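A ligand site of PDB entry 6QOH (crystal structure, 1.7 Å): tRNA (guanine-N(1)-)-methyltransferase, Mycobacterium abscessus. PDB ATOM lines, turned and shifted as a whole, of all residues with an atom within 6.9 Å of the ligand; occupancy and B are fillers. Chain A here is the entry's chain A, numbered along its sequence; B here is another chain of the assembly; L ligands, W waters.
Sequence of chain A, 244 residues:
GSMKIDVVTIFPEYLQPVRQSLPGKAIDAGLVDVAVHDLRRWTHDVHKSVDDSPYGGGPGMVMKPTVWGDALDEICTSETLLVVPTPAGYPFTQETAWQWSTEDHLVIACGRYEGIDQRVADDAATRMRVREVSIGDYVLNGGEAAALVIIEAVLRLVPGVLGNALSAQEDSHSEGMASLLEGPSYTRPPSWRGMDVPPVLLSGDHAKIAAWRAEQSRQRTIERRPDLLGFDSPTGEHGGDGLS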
ATOM      1  N   VAL A  84       7.576 -23.751  -9.463  1.00  0.00           N
ATOM      2  CA  VAL A  84       7.076 -24.599 -10.536  1.00  0.00           C
ATOM      3  C   VAL A  84       6.384 -23.740 -11.591  1.00  0.00           C
ATOM      4  O   VAL A  84       5.250 -23.308 -11.384  1.00  0.00           O
ATOM      5  CB  VAL A  84       6.088 -25.645 -10.022  1.00  0.00           C
ATOM      6  CG1 VAL A  84       5.692 -26.577 -11.164  1.00  0.00           C
ATOM      7  CG2 VAL A  84       6.677 -26.425  -8.858  1.00  0.00           C
ATOM      8  N   PRO A  85       7.064 -23.483 -12.722  1.00  0.00           N
ATOM      9  CA  PRO A  85       6.425 -22.731 -13.803  1.00  0.00           C
ATOM     10  C   PRO A  85       5.323 -23.518 -14.487  1.00  0.00           C
ATOM     11  O   PRO A  85       5.539 -24.635 -14.936  1.00  0.00           O
ATOM     12  CB  PRO A  85       7.583 -22.460 -14.780  1.00  0.00           C
ATOM     13  CG  PRO A  85       8.820 -22.577 -13.962  1.00  0.00           C
ATOM     14  CD  PRO A  85       8.512 -23.649 -12.947  1.00  0.00           C
ATOM     15  N   THR A  86       4.135 -22.925 -14.602  1.00  0.00           N
ATOM     16  CA  THR A  86       3.004 -23.627 -15.176  1.00  0.00           C
ATOM     17  C   THR A  86       1.991 -22.595 -15.631  1.00  0.00           C
ATOM     18  O   THR A  86       1.819 -21.573 -14.965  1.00  0.00           O
ATOM     19  CB  THR A  86       2.346 -24.596 -14.178  1.00  0.00           C
ATOM     20  OG1 THR A  86       1.061 -24.995 -14.661  1.00  0.00           O
ATOM     21  CG2 THR A  86       2.174 -23.946 -12.816  1.00  0.00           C
ATOM     22  N   PRO A  87       1.320 -22.861 -16.754  1.00  0.00           N
ATOM     23  CA  PRO A  87       0.331 -21.858 -17.196  1.00  0.00           C
ATOM     24  C   PRO A  87      -0.823 -21.732 -16.209  1.00  0.00           C
ATOM     25  O   PRO A  87      -1.558 -20.731 -16.229  1.00  0.00           O
ATOM     26  CB  PRO A  87      -0.150 -22.396 -18.553  1.00  0.00           C
ATOM     27  CG  PRO A  87       0.180 -23.826 -18.551  1.00  0.00           C
ATOM     28  CD  PRO A  87       1.355 -24.034 -17.641  1.00  0.00           C
ATOM     29  N   ALA A  88      -0.966 -22.725 -15.316  1.00  0.00           N
ATOM     30  CA  ALA A  88      -2.048 -22.728 -14.345  1.00  0.00           C
ATOM     31  C   ALA A  88      -1.623 -22.142 -12.995  1.00  0.00           C
ATOM     32  O   ALA A  88      -2.311 -22.352 -11.982  1.00  0.00           O
ATOM     33  CB  ALA A  88      -2.568 -24.164 -14.155  1.00  0.00           C
ATOM     34  N   GLY A  89      -0.509 -21.417 -12.981  1.00  0.00           N
ATOM     35  CA  GLY A  89       0.049 -20.899 -11.743  1.00  0.00           C
ATOM     36  C   GLY A  89      -0.588 -19.614 -11.226  1.00  0.00           C
ATOM     37  O   GLY A  89      -1.419 -19.000 -11.886  1.00  0.00           O
ATOM     38  N   GLY A 111       8.753 -28.319 -16.274  1.00  0.00           N
ATOM     39  CA  GLY A 111       8.037 -29.440 -16.850  1.00  0.00           C
ATOM     40  C   GLY A 111       7.241 -29.058 -18.081  1.00  0.00           C
ATOM     41  O   GLY A 111       7.102 -27.884 -18.427  1.00  0.00           O
ATOM     42  N   ARG A 112       6.722 -30.061 -18.780  1.00  0.00           N
ATOM     43  CA  ARG A 112       5.851 -29.790 -19.913  1.00  0.00           C
ATOM     44  C   ARG A 112       4.538 -29.157 -19.413  1.00  0.00           C
ATOM     45  O   ARG A 112       4.163 -29.341 -18.251  1.00  0.00           O
ATOM     46  CB  ARG A 112       5.574 -31.074 -20.691  1.00  0.00           C
ATOM     47  CG  ARG A 112       5.033 -32.202 -19.824  1.00  0.00           C
ATOM     48  CD  ARG A 112       5.037 -33.520 -20.614  1.00  0.00           C
ATOM     49  NE  ARG A 112       4.188 -33.445 -21.816  1.00  0.00           N
ATOM     50  CZ  ARG A 112       4.406 -34.131 -22.929  1.00  0.00           C
ATOM     51  NH1 ARG A 112       5.458 -34.939 -23.026  1.00  0.00           N
ATOM     52  NH2 ARG A 112       3.586 -34.006 -23.961  1.00  0.00           N
ATOM     53  N   TYR A 113       3.835 -28.428 -20.286  1.00  0.00           N
ATOM     54  CA  TYR A 113       2.709 -27.632 -19.824  1.00  0.00           C
ATOM     55  C   TYR A 113       1.525 -28.468 -19.343  1.00  0.00           C
ATOM     56  O   TYR A 113       0.763 -28.007 -18.480  1.00  0.00           O
ATOM     57  CB  TYR A 113       2.234 -26.668 -20.921  1.00  0.00           C
ATOM     58  CG  TYR A 113       1.342 -27.262 -21.970  1.00  0.00           C
ATOM     59  CD1 TYR A 113       1.879 -27.936 -23.061  1.00  0.00           C
ATOM     60  CD2 TYR A 113      -0.035 -27.143 -21.880  1.00  0.00           C
ATOM     61  CE1 TYR A 113       1.051 -28.472 -24.043  1.00  0.00           C
ATOM     62  CE2 TYR A 113      -0.868 -27.677 -22.848  1.00  0.00           C
ATOM     63  CZ  TYR A 113      -0.314 -28.344 -23.925  1.00  0.00           C
ATOM     64  OH  TYR A 113      -1.141 -28.885 -24.890  1.00  0.00           O
ATOM     65  N   GLU A 114       1.368 -29.691 -19.858  1.00  0.00           N
ATOM     66  CA  GLU A 114       0.310 -30.585 -19.369  1.00  0.00           C
ATOM     67  C   GLU A 114       0.458 -30.893 -17.871  1.00  0.00           C
ATOM     68  O   GLU A 114      -0.523 -31.238 -17.211  1.00  0.00           O
ATOM     69  CB  GLU A 114       0.293 -31.910 -20.136  1.00  0.00           C
ATOM     70  CG  GLU A 114      -0.018 -31.784 -21.614  1.00  0.00           C
ATOM     71  CD  GLU A 114       1.229 -31.781 -22.466  1.00  0.00           C
ATOM     72  OE1 GLU A 114       2.307 -31.376 -21.958  1.00  0.00           O
ATOM     73  OE2 GLU A 114       1.143 -32.209 -23.641  1.00  0.00           O
ATOM     74  N   VAL A 133       3.688 -20.940 -10.420  1.00  0.00           N
ATOM     75  CA  VAL A 133       3.503 -19.589 -10.979  1.00  0.00           C
ATOM     76  C   VAL A 133       3.463 -19.561 -12.497  1.00  0.00           C
ATOM     77  O   VAL A 133       4.113 -20.372 -13.173  1.00  0.00           O
ATOM     78  CB  VAL A 133       4.617 -18.619 -10.513  1.00  0.00           C
ATOM     79  CG1 VAL A 133       4.593 -18.448  -8.991  1.00  0.00           C
ATOM     80  CG2 VAL A 133       5.999 -19.088 -10.995  1.00  0.00           C
ATOM     81  N   SER A 134       2.690 -18.620 -13.038  1.00  0.00           N
ATOM     82  CA  SER A 134       2.704 -18.360 -14.483  1.00  0.00           C
ATOM     83  C   SER A 134       3.330 -16.997 -14.750  1.00  0.00           C
ATOM     84  O   SER A 134       3.235 -16.095 -13.920  1.00  0.00           O
ATOM     85  CB  SER A 134       1.288 -18.405 -15.042  1.00  0.00           C
ATOM     86  OG  SER A 134       0.521 -17.356 -14.476  1.00  0.00           O
ATOM     87  N   ILE A 135       3.971 -16.838 -15.901  1.00  0.00           N
ATOM     88  CA  ILE A 135       4.573 -15.554 -16.232  1.00  0.00           C
ATOM     89  C   ILE A 135       3.721 -14.733 -17.205  1.00  0.00           C
ATOM     90  O   ILE A 135       4.112 -13.634 -17.613  1.00  0.00           O
ATOM     91  CB  ILE A 135       5.986 -15.707 -16.831  1.00  0.00           C
ATOM     92  CG1 ILE A 135       5.980 -16.570 -18.098  1.00  0.00           C
ATOM     93  CG2 ILE A 135       6.952 -16.285 -15.782  1.00  0.00           C
ATOM     94  CD1 ILE A 135       7.200 -16.324 -18.975  1.00  0.00           C
ATOM     95  N   GLY A 136       2.535 -15.229 -17.571  1.00  0.00           N
ATOM     96  CA  GLY A 136       1.648 -14.458 -18.414  1.00  0.00           C
ATOM     97  C   GLY A 136       0.513 -15.272 -19.008  1.00  0.00           C
ATOM     98  O   GLY A 136       0.366 -16.465 -18.699  1.00  0.00           O
ATOM     99  N   ASP A 137      -0.291 -14.620 -19.839  1.00  0.00           N
ATOM    100  CA  ASP A 137      -1.507 -15.213 -20.355  1.00  0.00           C
ATOM    101  C   ASP A 137      -1.285 -15.757 -21.754  1.00  0.00           C
ATOM    102  O   ASP A 137      -1.812 -15.235 -22.729  1.00  0.00           O
ATOM    103  CB  ASP A 137      -2.639 -14.182 -20.404  1.00  0.00           C
ATOM    104  CG  ASP A 137      -2.988 -13.645 -19.029  1.00  0.00           C
ATOM    105  OD1 ASP A 137      -3.082 -14.446 -18.083  1.00  0.00           O
ATOM    106  OD2 ASP A 137      -3.175 -12.410 -18.906  1.00  0.00           O
ATOM    107  N   TYR A 138      -0.485 -16.810 -21.840  1.00  0.00           N
ATOM    108  CA  TYR A 138      -0.187 -17.499 -23.095  1.00  0.00           C
ATOM    109  C   TYR A 138       0.355 -18.839 -22.639  1.00  0.00           C
ATOM    110  O   TYR A 138       0.768 -18.982 -21.487  1.00  0.00           O
ATOM    111  CB  TYR A 138       0.838 -16.741 -23.955  1.00  0.00           C
ATOM    112  CG  TYR A 138       1.913 -16.080 -23.113  1.00  0.00           C
ATOM    113  CD1 TYR A 138       2.955 -16.839 -22.569  1.00  0.00           C
ATOM    114  CD2 TYR A 138       1.853 -14.723 -22.810  1.00  0.00           C
ATOM    115  CE1 TYR A 138       3.898 -16.262 -21.759  1.00  0.00           C
ATOM    116  CE2 TYR A 138       2.816 -14.126 -21.994  1.00  0.00           C
ATOM    117  CZ  TYR A 138       3.834 -14.916 -21.472  1.00  0.00           C
ATOM    118  OH  TYR A 138       4.787 -14.358 -20.663  1.00  0.00           O
ATOM    119  N   VAL A 139       0.330 -19.821 -23.543  1.00  0.00           N
ATOM    120  CA  VAL A 139       0.831 -21.136 -23.193  1.00  0.00           C
ATOM    121  C   VAL A 139       2.181 -21.395 -23.877  1.00  0.00           C
ATOM    122  O   VAL A 139       2.340 -21.157 -25.069  1.00  0.00           O
ATOM    123  CB  VAL A 139      -0.174 -22.254 -23.609  1.00  0.00           C
ATOM    124  CG1 VAL A 139       0.414 -23.637 -23.322  1.00  0.00           C
ATOM    125  CG2 VAL A 139      -1.480 -22.080 -22.865  1.00  0.00           C
ATOM    126  N   LEU A 140       3.128 -21.909 -23.092  1.00  0.00           N
ATOM    127  CA  LEU A 140       4.399 -22.396 -23.621  1.00  0.00           C
ATOM    128  C   LEU A 140       4.375 -23.905 -23.547  1.00  0.00           C
ATOM    129  O   LEU A 140       3.696 -24.457 -22.685  1.00  0.00           O
ATOM    130  CB  LEU A 140       5.586 -21.868 -22.815  1.00  0.00           C
ATOM    131  CG  LEU A 140       5.642 -20.372 -22.540  1.00  0.00           C
ATOM    132  CD1 LEU A 140       6.815 -20.022 -21.619  1.00  0.00           C
ATOM    133  CD2 LEU A 140       5.705 -19.575 -23.848  1.00  0.00           C
ATOM    134  N   ASN A 141       5.102 -24.571 -24.432  1.00  0.00           N
ATOM    135  CA  ASN A 141       5.128 -26.027 -24.420  1.00  0.00           C
ATOM    136  C   ASN A 141       5.736 -26.591 -23.126  1.00  0.00           C
ATOM    137  O   ASN A 141       5.402 -27.703 -22.699  1.00  0.00           O
ATOM    138  CB  ASN A 141       5.913 -26.565 -25.597  1.00  0.00           C
ATOM    139  CG  ASN A 141       5.156 -27.627 -26.354  1.00  0.00           C
ATOM    140  OD1 ASN A 141       3.990 -27.435 -26.707  1.00  0.00           O
ATOM    141  ND2 ASN A 141       5.797 -28.777 -26.567  1.00  0.00           N
ATOM    142  N   GLY A 142       6.647 -25.839 -22.529  1.00  0.00           N
ATOM    143  CA  GLY A 142       7.294 -26.265 -21.304  1.00  0.00           C
ATOM    144  C   GLY A 142       7.753 -25.057 -20.508  1.00  0.00           C
ATOM    145  O   GLY A 142       7.727 -23.929 -21.001  1.00  0.00           O
ATOM    146  N   GLY A 143       8.169 -25.294 -19.267  1.00  0.00           N
ATOM    147  CA  GLY A 143       8.505 -24.187 -18.381  1.00  0.00           C
ATOM    148  C   GLY A 143       9.888 -23.568 -18.563  1.00  0.00           C
ATOM    149  O   GLY A 143      10.195 -22.589 -17.893  1.00  0.00           O
ATOM    150  N   GLU A 144      10.693 -24.111 -19.468  1.00  0.00           N
ATOM    151  CA  GLU A 144      12.077 -23.652 -19.639  1.00  0.00           C
ATOM    152  C   GLU A 144      12.216 -22.149 -19.925  1.00  0.00           C
ATOM    153  O   GLU A 144      12.964 -21.447 -19.239  1.00  0.00           O
ATOM    154  CB  GLU A 144      12.765 -24.456 -20.742  1.00  0.00           C
ATOM    155  CG  GLU A 144      13.253 -25.842 -20.288  1.00  0.00           C
ATOM    156  CD  GLU A 144      12.134 -26.865 -20.105  1.00  0.00           C
ATOM    157  OE1 GLU A 144      11.019 -26.652 -20.648  1.00  0.00           O
ATOM    158  OE2 GLU A 144      12.371 -27.907 -19.453  1.00  0.00           O
ATOM    159  N   ALA A 146      10.083 -19.832 -19.376  1.00  0.00           N
ATOM    160  CA  ALA A 146       9.572 -19.120 -18.192  1.00  0.00           C
ATOM    161  C   ALA A 146      10.616 -19.058 -17.100  1.00  0.00           C
ATOM    162  O   ALA A 146      10.750 -18.051 -16.391  1.00  0.00           O
ATOM    163  CB  ALA A 146       8.299 -19.782 -17.685  1.00  0.00           C
ATOM    164  N   ALA A 147      11.353 -20.151 -16.929  1.00  0.00           N
ATOM    165  CA  ALA A 147      12.417 -20.178 -15.941  1.00  0.00           C
ATOM    166  C   ALA A 147      13.476 -19.139 -16.244  1.00  0.00           C
ATOM    167  O   ALA A 147      13.990 -18.480 -15.329  1.00  0.00           O
ATOM    168  CB  ALA A 147      13.054 -21.571 -15.871  1.00  0.00           C
ATOM    169  N   ILE A 150      12.000 -15.794 -15.125  1.00  0.00           N
ATOM    170  CA  ILE A 150      12.042 -15.723 -13.664  1.00  0.00           C
ATOM    171  C   ILE A 150      13.464 -15.514 -13.122  1.00  0.00           C
ATOM    172  O   ILE A 150      13.695 -14.668 -12.251  1.00  0.00           O
ATOM    173  CB  ILE A 150      11.433 -17.001 -13.050  1.00  0.00           C
ATOM    174  CG1 ILE A 150       9.933 -17.051 -13.358  1.00  0.00           C
ATOM    175  CG2 ILE A 150      11.704 -17.063 -11.543  1.00  0.00           C
ATOM    176  CD1 ILE A 150       9.269 -18.423 -13.075  1.00  0.00           C
ATOM    177  N   VAL B 149      10.407 -16.360 -25.114  1.00  0.00           N
ATOM    178  CA  VAL B 149       9.022 -16.660 -24.729  1.00  0.00           C
ATOM    179  C   VAL B 149       8.070 -16.467 -25.912  1.00  0.00           C
ATOM    180  O   VAL B 149       7.231 -17.330 -26.200  1.00  0.00           O
ATOM    181  CB  VAL B 149       8.582 -15.757 -23.560  1.00  0.00           C
ATOM    182  CG1 VAL B 149       7.051 -15.769 -23.389  1.00  0.00           C
ATOM    183  CG2 VAL B 149       9.285 -16.218 -22.275  1.00  0.00           C
HETATM  184 CL1  LIG L   1       5.384 -20.506 -16.056  1.00  0.00          CL
HETATM  185  N1  LIG L   1       4.952 -22.416 -18.014  1.00  0.00           N
HETATM  186  C1  LIG L   1       4.355 -22.783 -19.187  1.00  0.00           C
HETATM  187  N2  LIG L   1       4.573 -24.079 -19.723  1.00  0.00           N
HETATM  188  N3  LIG L   1       3.570 -21.930 -19.863  1.00  0.00           N
HETATM  189  C2  LIG L   1       3.323 -20.664 -19.397  1.00  0.00           C
HETATM  190  C3  LIG L   1       3.908 -20.289 -18.216  1.00  0.00           C
HETATM  191  C4  LIG L   1       4.724 -21.177 -17.522  1.00  0.00           C
HETATM  192  N4  LIG L   1       3.549 -19.000 -17.911  1.00  0.00           N
HETATM  193  C5  LIG L   1       2.739 -18.587 -18.911  1.00  0.00           C
HETATM  194  N5  LIG L   1       2.602 -19.579 -19.816  1.00  0.00           N
HETATM  195  O   HOH W   1       5.041 -25.963 -17.558  1.00  0.00           O
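Pro 85 touches the ligand (CB to CL1, 3.2 Å).
N of Thr 86 touches CL1 of the ligand, 3.1 Å away.
Pro 87 touches the ligand.
Tyr 113 touches the ligand.
O of Val 133 touches CL1 of the ligand, at 3.2 Å.
CA of Ser 134 touches N4 of the ligand, 3.6 Å away.
O of Gly 136 touches C5 of the ligand, 3.2 Å away.
Gly 143 touches the ligand.
Ala 146 touches the ligand (CB to CL1, 3.4 Å).
Hydrophobic or aromatic side chains that line the ligand: Pro 85, Pro 87, Tyr 113, Ile 135, Tyr 138, Leu 140 and Ala 146.
13 residues have an atom within 4 Å of the ligand: Pro 85, Thr 86, Pro 87, Tyr 113, Val 133, Ser 134, Ile 135, Gly 136, Tyr 138, Leu 140, Gly 142, Gly 143 and Ala 146.
The nearest printed residue that does not touch the ligand is Val 139 (4.1 Å).
The side-chain hydroxyl (OH) of Tyr 138 lies within hydrogen-bond range of the backbone carbonyl oxygen (O) of Ile 135, at 3.2 Å.
The backbone NH (N) of Thr 86 is in hydrogen-bond range of the backbone carbonyl oxygen (O) of Val 133 (2.9 Å).
The backbone NH of Ala 88 lies close to the side-chain hydroxyl of Thr 86 (3.1 Å).
O of Val 84 is in hydrogen-bond range of N of Val 133, at 3.0 Å.
N of Tyr 113 sits at hydrogen-bond distance from O of Asn 141.
The backbone carbonyl oxygen (O) of Gly 111 sits at hydrogen-bond distance from the backbone NH (N) of Gly 143 (2.9 Å).
N5 of the ligand sits at hydrogen-bond distance from O of Tyr 138.
The backbone NH (N) of Ile 135 sits at hydrogen-bond distance from a nitrogen (N4) of the ligand.
N of Leu 140 is in hydrogen-bond range of N3 of the ligand, at 3.3 Å.
The backbone carbonyl oxygen (O) of Leu 140 sits at hydrogen-bond distance from a nitrogen (N2) of the ligand.
The backbone carbonyl oxygen (O) of Gly 142 lies within hydrogen-bond range of a nitrogen (N2) of the ligand (3.4 Å).
Water W1 lies within hydrogen-bond range of a nitrogen (N2) of the ligand (2.9 Å), the backbone carbonyl oxygen of Gly 111 (2.9 Å) and the backbone carbonyl oxygen of Pro 85 (3.0 Å).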
